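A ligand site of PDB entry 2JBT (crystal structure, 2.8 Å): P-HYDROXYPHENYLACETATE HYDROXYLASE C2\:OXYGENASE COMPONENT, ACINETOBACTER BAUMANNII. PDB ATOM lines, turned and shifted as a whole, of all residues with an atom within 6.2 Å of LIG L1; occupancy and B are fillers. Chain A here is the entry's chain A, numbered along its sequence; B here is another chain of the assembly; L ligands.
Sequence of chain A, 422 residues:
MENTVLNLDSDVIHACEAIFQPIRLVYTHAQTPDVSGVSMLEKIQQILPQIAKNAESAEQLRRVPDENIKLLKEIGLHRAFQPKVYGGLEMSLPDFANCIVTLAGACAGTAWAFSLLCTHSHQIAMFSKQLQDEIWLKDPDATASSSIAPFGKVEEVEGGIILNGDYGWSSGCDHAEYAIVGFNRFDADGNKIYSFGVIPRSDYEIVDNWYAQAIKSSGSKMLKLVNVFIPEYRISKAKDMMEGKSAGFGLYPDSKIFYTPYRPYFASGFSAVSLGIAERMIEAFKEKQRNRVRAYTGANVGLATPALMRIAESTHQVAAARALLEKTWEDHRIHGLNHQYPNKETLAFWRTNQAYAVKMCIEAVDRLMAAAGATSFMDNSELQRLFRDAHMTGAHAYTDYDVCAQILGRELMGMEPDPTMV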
ATOM      1  N   LEU A 116       5.766   0.005  -0.706  1.00  0.00           N
ATOM      2  CA  LEU A 116       4.565   0.785  -0.911  1.00  0.00           C
ATOM      3  C   LEU A 116       3.305  -0.073  -0.884  1.00  0.00           C
ATOM      4  O   LEU A 116       2.343   0.263  -0.185  1.00  0.00           O
ATOM      5  CB  LEU A 116       4.666   1.579  -2.215  1.00  0.00           C
ATOM      6  CG  LEU A 116       5.584   2.792  -2.091  1.00  0.00           C
ATOM      7  CD1 LEU A 116       6.006   3.323  -3.432  1.00  0.00           C
ATOM      8  CD2 LEU A 116       4.918   3.870  -1.251  1.00  0.00           C
ATOM      9  N   THR A 119       2.783  -0.776   2.848  1.00  0.00           N
ATOM     10  CA  THR A 119       2.442   0.322   3.756  1.00  0.00           C
ATOM     11  C   THR A 119       1.079   0.897   3.457  1.00  0.00           C
ATOM     12  O   THR A 119       0.435   1.476   4.343  1.00  0.00           O
ATOM     13  CB  THR A 119       3.526   1.438   3.817  1.00  0.00           C
ATOM     14  OG1 THR A 119       3.644   2.103   2.553  1.00  0.00           O
ATOM     15  CG2 THR A 119       4.888   0.877   4.230  1.00  0.00           C
ATOM     16  N   HIS A 120       0.614   0.744   2.219  1.00  0.00           N
ATOM     17  CA  HIS A 120      -0.744   1.143   1.863  1.00  0.00           C
ATOM     18  C   HIS A 120      -1.798   0.388   2.675  1.00  0.00           C
ATOM     19  O   HIS A 120      -2.811   0.969   3.058  1.00  0.00           O
ATOM     20  CB  HIS A 120      -0.994   0.993   0.361  1.00  0.00           C
ATOM     21  CG  HIS A 120      -0.148   1.903  -0.486  1.00  0.00           C
ATOM     22  ND1 HIS A 120       0.290   1.552  -1.741  1.00  0.00           N
ATOM     23  CD2 HIS A 120       0.369   3.124  -0.232  1.00  0.00           C
ATOM     24  CE1 HIS A 120       1.012   2.529  -2.239  1.00  0.00           C
ATOM     25  NE2 HIS A 120       1.080   3.498  -1.349  1.00  0.00           N
ATOM     26  N   SER A 146      -0.573   3.335  -5.406  1.00  0.00           N
ATOM     27  CA  SER A 146      -1.079   4.680  -5.137  1.00  0.00           C
ATOM     28  C   SER A 146      -0.629   5.732  -6.135  1.00  0.00           C
ATOM     29  O   SER A 146       0.271   5.507  -6.916  1.00  0.00           O
ATOM     30  CB  SER A 146      -0.683   5.128  -3.733  1.00  0.00           C
ATOM     31  OG  SER A 146       0.701   5.410  -3.675  1.00  0.00           O
ATOM     32  N   SER A 147      -1.315   6.873  -6.083  1.00  0.00           N
ATOM     33  CA  SER A 147      -0.865   8.089  -6.732  1.00  0.00           C
ATOM     34  C   SER A 147      -1.516   9.211  -5.932  1.00  0.00           C
ATOM     35  O   SER A 147      -2.715   9.482  -6.079  1.00  0.00           O
ATOM     36  CB  SER A 147      -1.291   8.128  -8.207  1.00  0.00           C
ATOM     37  OG  SER A 147      -0.782   9.282  -8.842  1.00  0.00           O
ATOM     38  N   ILE A 148      -0.726   9.845  -5.063  1.00  0.00           N
ATOM     39  CA  ILE A 148      -1.275  10.678  -3.993  1.00  0.00           C
ATOM     40  C   ILE A 148      -1.349  12.187  -4.247  1.00  0.00           C
ATOM     41  O   ILE A 148      -2.157  12.882  -3.618  1.00  0.00           O
ATOM     42  CB  ILE A 148      -0.598  10.384  -2.633  1.00  0.00           C
ATOM     43  CG1 ILE A 148       0.809  10.971  -2.571  1.00  0.00           C
ATOM     44  CG2 ILE A 148      -0.585   8.887  -2.356  1.00  0.00           C
ATOM     45  CD1 ILE A 148       1.190  11.481  -1.196  1.00  0.00           C
ATOM     46  N   TYR A 194      -7.922  17.709   1.639  1.00  0.00           N
ATOM     47  CA  TYR A 194      -7.125  16.653   1.043  1.00  0.00           C
ATOM     48  C   TYR A 194      -7.648  15.280   1.462  1.00  0.00           C
ATOM     49  O   TYR A 194      -7.716  14.952   2.651  1.00  0.00           O
ATOM     50  CB  TYR A 194      -5.661  16.812   1.398  1.00  0.00           C
ATOM     51  CG  TYR A 194      -4.734  15.823   0.731  1.00  0.00           C
ATOM     52  CD1 TYR A 194      -4.892  15.484  -0.612  1.00  0.00           C
ATOM     53  CD2 TYR A 194      -3.661  15.263   1.431  1.00  0.00           C
ATOM     54  CE1 TYR A 194      -4.038  14.596  -1.233  1.00  0.00           C
ATOM     55  CE2 TYR A 194      -2.798  14.375   0.816  1.00  0.00           C
ATOM     56  CZ  TYR A 194      -2.989  14.044  -0.512  1.00  0.00           C
ATOM     57  OH  TYR A 194      -2.135  13.171  -1.130  1.00  0.00           O
ATOM     58  N   PHE A 196      -8.290  10.875   0.322  1.00  0.00           N
ATOM     59  CA  PHE A 196      -7.854   9.678  -0.368  1.00  0.00           C
ATOM     60  C   PHE A 196      -9.030   8.812  -0.718  1.00  0.00           C
ATOM     61  O   PHE A 196      -9.887   8.543   0.132  1.00  0.00           O
ATOM     62  CB  PHE A 196      -6.884   8.875   0.498  1.00  0.00           C
ATOM     63  CG  PHE A 196      -5.581   9.554   0.747  1.00  0.00           C
ATOM     64  CD1 PHE A 196      -4.601   9.624  -0.253  1.00  0.00           C
ATOM     65  CD2 PHE A 196      -5.313  10.131   1.988  1.00  0.00           C
ATOM     66  CE1 PHE A 196      -3.397  10.261  -0.018  1.00  0.00           C
ATOM     67  CE2 PHE A 196      -4.101  10.769   2.229  1.00  0.00           C
ATOM     68  CZ  PHE A 196      -3.141  10.831   1.222  1.00  0.00           C
ATOM     69  N   TYR A 262      -1.127   8.052   9.755  1.00  0.00           N
ATOM     70  CA  TYR A 262      -0.936   7.157   8.629  1.00  0.00           C
ATOM     71  C   TYR A 262       0.389   7.455   7.940  1.00  0.00           C
ATOM     72  O   TYR A 262       1.089   6.545   7.524  1.00  0.00           O
ATOM     73  CB  TYR A 262      -2.118   7.294   7.643  1.00  0.00           C
ATOM     74  CG  TYR A 262      -1.995   8.443   6.682  1.00  0.00           C
ATOM     75  CD1 TYR A 262      -1.409   8.266   5.410  1.00  0.00           C
ATOM     76  CD2 TYR A 262      -2.397   9.713   7.043  1.00  0.00           C
ATOM     77  CE1 TYR A 262      -1.247   9.336   4.531  1.00  0.00           C
ATOM     78  CE2 TYR A 262      -2.249  10.804   6.168  1.00  0.00           C
ATOM     79  CZ  TYR A 262      -1.680  10.599   4.922  1.00  0.00           C
ATOM     80  OH  TYR A 262      -1.520  11.658   4.065  1.00  0.00           O
ATOM     81  N   ARG A 263       0.752   8.738   7.843  1.00  0.00           N
ATOM     82  CA  ARG A 263       1.772   9.159   6.877  1.00  0.00           C
ATOM     83  C   ARG A 263       3.189   8.629   7.187  1.00  0.00           C
ATOM     84  O   ARG A 263       3.875   8.155   6.260  1.00  0.00           O
ATOM     85  CB  ARG A 263       1.755  10.654   6.683  1.00  0.00           C
ATOM     86  CG  ARG A 263       2.450  11.103   5.428  1.00  0.00           C
ATOM     87  CD  ARG A 263       2.301  12.623   5.275  1.00  0.00           C
ATOM     88  NE  ARG A 263       3.022  13.136   4.114  1.00  0.00           N
ATOM     89  CZ  ARG A 263       3.547  14.357   4.037  1.00  0.00           C
ATOM     90  NH1 ARG A 263       3.440  15.187   5.082  1.00  0.00           N
ATOM     91  NH2 ARG A 263       4.199  14.751   2.940  1.00  0.00           N
ATOM     92  N   PHE A 266       3.178   5.160   5.877  1.00  0.00           N
ATOM     93  CA  PHE A 266       3.021   5.381   4.439  1.00  0.00           C
ATOM     94  C   PHE A 266       4.383   5.546   3.777  1.00  0.00           C
ATOM     95  O   PHE A 266       4.756   4.789   2.878  1.00  0.00           O
ATOM     96  CB  PHE A 266       2.194   6.667   4.238  1.00  0.00           C
ATOM     97  CG  PHE A 266       1.169   6.586   3.139  1.00  0.00           C
ATOM     98  CD1 PHE A 266       0.248   5.521   3.066  1.00  0.00           C
ATOM     99  CD2 PHE A 266       1.058   7.623   2.204  1.00  0.00           C
ATOM    100  CE1 PHE A 266      -0.714   5.478   2.059  1.00  0.00           C
ATOM    101  CE2 PHE A 266       0.103   7.583   1.185  1.00  0.00           C
ATOM    102  CZ  PHE A 266      -0.798   6.512   1.116  1.00  0.00           C
ATOM    103  N   ALA A 267       5.136   6.522   4.277  1.00  0.00           N
ATOM    104  CA  ALA A 267       6.370   6.996   3.650  1.00  0.00           C
ATOM    105  C   ALA A 267       7.656   6.491   4.337  1.00  0.00           C
ATOM    106  O   ALA A 267       8.729   7.065   4.138  1.00  0.00           O
ATOM    107  CB  ALA A 267       6.370   8.512   3.618  1.00  0.00           C
ATOM    108  N   PHE A 270      10.979   4.778   1.842  1.00  0.00           N
ATOM    109  CA  PHE A 270      11.925   5.473   0.955  1.00  0.00           C
ATOM    110  C   PHE A 270      13.305   5.429   1.541  1.00  0.00           C
ATOM    111  O   PHE A 270      14.237   4.917   0.917  1.00  0.00           O
ATOM    112  CB  PHE A 270      11.520   6.917   0.678  1.00  0.00           C
ATOM    113  CG  PHE A 270      10.091   7.067   0.233  1.00  0.00           C
ATOM    114  CD1 PHE A 270       9.600   6.344  -0.834  1.00  0.00           C
ATOM    115  CD2 PHE A 270       9.253   7.964   0.884  1.00  0.00           C
ATOM    116  CE1 PHE A 270       8.279   6.496  -1.244  1.00  0.00           C
ATOM    117  CE2 PHE A 270       7.930   8.131   0.476  1.00  0.00           C
ATOM    118  CZ  PHE A 270       7.445   7.399  -0.581  1.00  0.00           C
ATOM    119  N   ARG A 351       8.828  13.286  10.403  1.00  0.00           N
ATOM    120  CA  ARG A 351       8.634  13.714   9.035  1.00  0.00           C
ATOM    121  C   ARG A 351       9.992  13.914   8.344  1.00  0.00           C
ATOM    122  O   ARG A 351      10.136  13.658   7.146  1.00  0.00           O
ATOM    123  CB  ARG A 351       7.782  14.980   9.002  1.00  0.00           C
ATOM    124  CG  ARG A 351       7.755  15.725   7.673  1.00  0.00           C
ATOM    125  CD  ARG A 351       6.889  15.034   6.620  1.00  0.00           C
ATOM    126  NE  ARG A 351       6.971  15.727   5.340  1.00  0.00           N
ATOM    127  CZ  ARG A 351       7.935  15.509   4.439  1.00  0.00           C
ATOM    128  NH1 ARG A 351       8.894  14.605   4.663  1.00  0.00           N
ATOM    129  NH2 ARG A 351       7.940  16.199   3.298  1.00  0.00           N
ATOM    130  N   HIS A 396      12.410  11.715  -4.512  1.00  0.00           N
ATOM    131  CA  HIS A 396      11.007  11.701  -4.130  1.00  0.00           C
ATOM    132  C   HIS A 396      10.636  12.973  -3.388  1.00  0.00           C
ATOM    133  O   HIS A 396      11.428  13.500  -2.604  1.00  0.00           O
ATOM    134  CB  HIS A 396      10.746  10.510  -3.233  1.00  0.00           C
ATOM    135  CG  HIS A 396       9.294  10.214  -3.056  1.00  0.00           C
ATOM    136  ND1 HIS A 396       8.507  10.885  -2.144  1.00  0.00           N
ATOM    137  CD2 HIS A 396       8.484   9.319  -3.667  1.00  0.00           C
ATOM    138  CE1 HIS A 396       7.279  10.413  -2.200  1.00  0.00           C
ATOM    139  NE2 HIS A 396       7.233   9.467  -3.123  1.00  0.00           N
ATOM    140  N   TYR A 398       8.953  13.389  -0.893  1.00  0.00           N
ATOM    141  CA  TYR A 398       8.919  13.209   0.552  1.00  0.00           C
ATOM    142  C   TYR A 398      10.331  13.192   1.165  1.00  0.00           C
ATOM    143  O   TYR A 398      10.478  13.359   2.382  1.00  0.00           O
ATOM    144  CB  TYR A 398       8.186  11.913   0.896  1.00  0.00           C
ATOM    145  CG  TYR A 398       7.849  11.772   2.354  1.00  0.00           C
ATOM    146  CD1 TYR A 398       6.712  12.380   2.878  1.00  0.00           C
ATOM    147  CD2 TYR A 398       8.657  11.042   3.219  1.00  0.00           C
ATOM    148  CE1 TYR A 398       6.376  12.275   4.224  1.00  0.00           C
ATOM    149  CE2 TYR A 398       8.346  10.936   4.581  1.00  0.00           C
ATOM    150  CZ  TYR A 398       7.194  11.557   5.073  1.00  0.00           C
ATOM    151  OH  TYR A 398       6.852  11.424   6.409  1.00  0.00           O
ATOM    152  N   VAL A 422       4.601  20.401   2.614  1.00  0.00           N
ATOM    153  CA  VAL A 422       3.937  19.503   3.547  1.00  0.00           C
ATOM    154  C   VAL A 422       4.741  18.201   3.746  1.00  0.00           C
ATOM    155  O   VAL A 422       4.780  17.592   4.824  1.00  0.00           O
ATOM    156  CB  VAL A 422       2.444  19.269   3.121  1.00  0.00           C
ATOM    157  CG1 VAL A 422       2.350  18.390   1.867  1.00  0.00           C
ATOM    158  CG2 VAL A 422       1.603  18.717   4.282  1.00  0.00           C
ATOM    159  OXT VAL A 422       5.411  17.738   2.828  1.00  0.00           O
ATOM    160  N   TYR B 296       2.563  18.124  -4.131  1.00  0.00           N
ATOM    161  CA  TYR B 296       1.702  17.939  -2.971  1.00  0.00           C
ATOM    162  C   TYR B 296       0.870  19.167  -2.570  1.00  0.00           C
ATOM    163  O   TYR B 296      -0.240  19.012  -2.044  1.00  0.00           O
ATOM    164  CB  TYR B 296       2.514  17.454  -1.760  1.00  0.00           C
ATOM    165  CG  TYR B 296       3.165  16.100  -1.921  1.00  0.00           C
ATOM    166  CD1 TYR B 296       2.698  15.169  -2.870  1.00  0.00           C
ATOM    167  CD2 TYR B 296       4.230  15.726  -1.103  1.00  0.00           C
ATOM    168  CE1 TYR B 296       3.295  13.927  -2.995  1.00  0.00           C
ATOM    169  CE2 TYR B 296       4.832  14.479  -1.236  1.00  0.00           C
ATOM    170  CZ  TYR B 296       4.353  13.589  -2.182  1.00  0.00           C
ATOM    171  OH  TYR B 296       4.954  12.355  -2.312  1.00  0.00           O
HETATM  172  C1  LIG L   1       3.427  11.423   1.439  1.00  0.00           C
HETATM  173  O1  LIG L   1       2.525  10.887   2.118  1.00  0.00           O
HETATM  174  O2  LIG L   1       3.428  12.647   1.199  1.00  0.00           O
HETATM  175  C2  LIG L   1       4.550  10.577   0.865  1.00  0.00           C
HETATM  176  C3  LIG L   1       4.014   9.313   0.228  1.00  0.00           C
HETATM  177  C4  LIG L   1       3.775   8.177   0.998  1.00  0.00           C
HETATM  178  C5  LIG L   1       3.277   7.016   0.402  1.00  0.00           C
HETATM  179  C6  LIG L   1       3.010   7.013  -0.972  1.00  0.00           C
HETATM  180  C7  LIG L   1       3.261   8.143  -1.745  1.00  0.00           C
HETATM  181  C8  LIG L   1       3.769   9.304  -1.143  1.00  0.00           C
HETATM  182  O3  LIG L   1       2.521   5.888  -1.562  1.00  0.00           O
HETATM  183  N1  LG2 L   2       3.994   8.926  -5.692  1.00  0.00           N
HETATM  184  C1  LG2 L   2       2.840   8.247  -5.390  1.00  0.00           C
HETATM  185  O1  LG2 L   2       1.862   8.891  -5.021  1.00  0.00           O
HETATM  186  N2  LG2 L   2       2.801   6.866  -5.512  1.00  0.00           N
HETATM  187  C2  LG2 L   2       3.921   6.172  -5.940  1.00  0.00           C
HETATM  188  O2  LG2 L   2       3.898   4.936  -5.983  1.00  0.00           O
HETATM  189  C3  LG2 L   2       5.111   6.861  -6.242  1.00  0.00           C
HETATM  190  N3  LG2 L   2       6.253   6.197  -6.665  1.00  0.00           N
HETATM  191  C4  LG2 L   2       7.400   6.923  -6.951  1.00  0.00           C
HETATM  192  C5  LG2 L   2       8.538   6.251  -7.370  1.00  0.00           C
HETATM  193  C6  LG2 L   2       9.712   6.952  -7.663  1.00  0.00           C
HETATM  194  C7  LG2 L   2      10.969   6.154  -7.941  1.00  0.00           C
HETATM  195  C8  LG2 L   2       9.758   8.343  -7.516  1.00  0.00           C
HETATM  196  C9  LG2 L   2      11.088   9.004  -7.236  1.00  0.00           C
HETATM  197  C10 LG2 L   2       8.598   9.021  -7.100  1.00  0.00           C
HETATM  198  C11 LG2 L   2       7.425   8.321  -6.808  1.00  0.00           C
HETATM  199  N4  LG2 L   2       6.279   8.990  -6.377  1.00  0.00           N
HETATM  200  C12 LG2 L   2       5.137   8.259  -6.098  1.00  0.00           C
HETATM  201  C13 LG2 L   2       6.071  10.423  -6.779  1.00  0.00           C
HETATM  202  C14 LG2 L   2       6.097  11.354  -5.564  1.00  0.00           C
HETATM  203  O3  LG2 L   2       5.070  11.038  -4.655  1.00  0.00           O
HETATM  204  C15 LG2 L   2       5.924  12.801  -5.983  1.00  0.00           C
HETATM  205  O4  LG2 L   2       4.620  12.988  -6.493  1.00  0.00           O
HETATM  206  C16 LG2 L   2       6.984  13.168  -6.996  1.00  0.00           C
HETATM  207  O5  LG2 L   2       8.257  13.091  -6.393  1.00  0.00           O
HETATM  208  C17 LG2 L   2       6.773  14.571  -7.545  1.00  0.00           C
HETATM  209  O6  LG2 L   2       7.936  15.311  -7.259  1.00  0.00           O
HETATM  210  P1  LG2 L   2       8.662  16.154  -8.405  1.00  0.00           P
HETATM  211  O7  LG2 L   2       9.593  15.310  -8.957  1.00  0.00           O
HETATM  212  O8  LG2 L   2       7.945  16.801  -9.138  1.00  0.00           O
HETATM  213  O9  LG2 L   2       9.307  16.975  -7.781  1.00  0.00           O
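CD2 of Leu 116 touches O3 of LIG L1 (3.1 Å). Ile 148 touches LIG L1 (CD1 to C8, 3.4 Å). Phe 266 touches LIG L1 (CD2 to C5, 2.9 Å). Ala 267 touches LIG L1. His 396 touches LIG L1. CD1 of Tyr 398 touches C2 of LIG L1, 3.5 Å away. CE2 of Tyr 296 of chain B touches O2 of LIG L1, at 3.4 Å. The nearest printed residue that does not touch LIG L1 is Phe 270 (4.01 Å).
O of Tyr 398 is in hydrogen-bond range of NH1 of Arg 351. The guanidinium group of Arg 263 is in salt-bridge range of the chain-end carboxylate of Val 422. A ring nitrogen (ND1) of His 120 lies within hydrogen-bond range of the backbone carbonyl oxygen (O) of Leu 116 (2.9 Å). N of Tyr 398 is in hydrogen-bond range of ND1 of His 396, 2.8 Å away. A ring nitrogen (NE2) of His 120 sits at hydrogen-bond distance from the side-chain hydroxyl (OG) of Ser 146, at 3.0 Å. The side-chain hydroxyl of Thr 119 sits at hydrogen-bond distance from the backbone carbonyl oxygen of Phe 266 (2.9 Å). The backbone carbonyl oxygen (O) of Ile 148 sits at hydrogen-bond distance from the side-chain hydroxyl (OH) of Tyr 194.
O3 of LG2 L2 sits at hydrogen-bond distance from NE2 of His 396, at 3.1 Å. An oxygen (O2) of LIG L1 is in salt-bridge range of the guanidinium group (NH2) of Arg 263 (2.8 Å). A nitrogen (N2) of LG2 L2 lies within hydrogen-bond range of the backbone carbonyl oxygen of Ser 146 (3.2 Å). NE2 of His 120 lies within hydrogen-bond range of O3 of LIG L1 (2.8 Å). N of Ile 148 lies within hydrogen-bond range of O1 of LG2 L2 (2.8 Å). An oxygen (O3) of LG2 L2 sits at hydrogen-bond distance from the side-chain hydroxyl (OH) of Tyr 296 of chain B (2.7 Å). An oxygen (O3) of LIG L1 sits at hydrogen-bond distance from the side-chain hydroxyl (OG) of Ser 146, 2.8 Å away. A nitrogen (N2) of LG2 L2 sits at hydrogen-bond distance from the side-chain hydroxyl of Ser 146.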
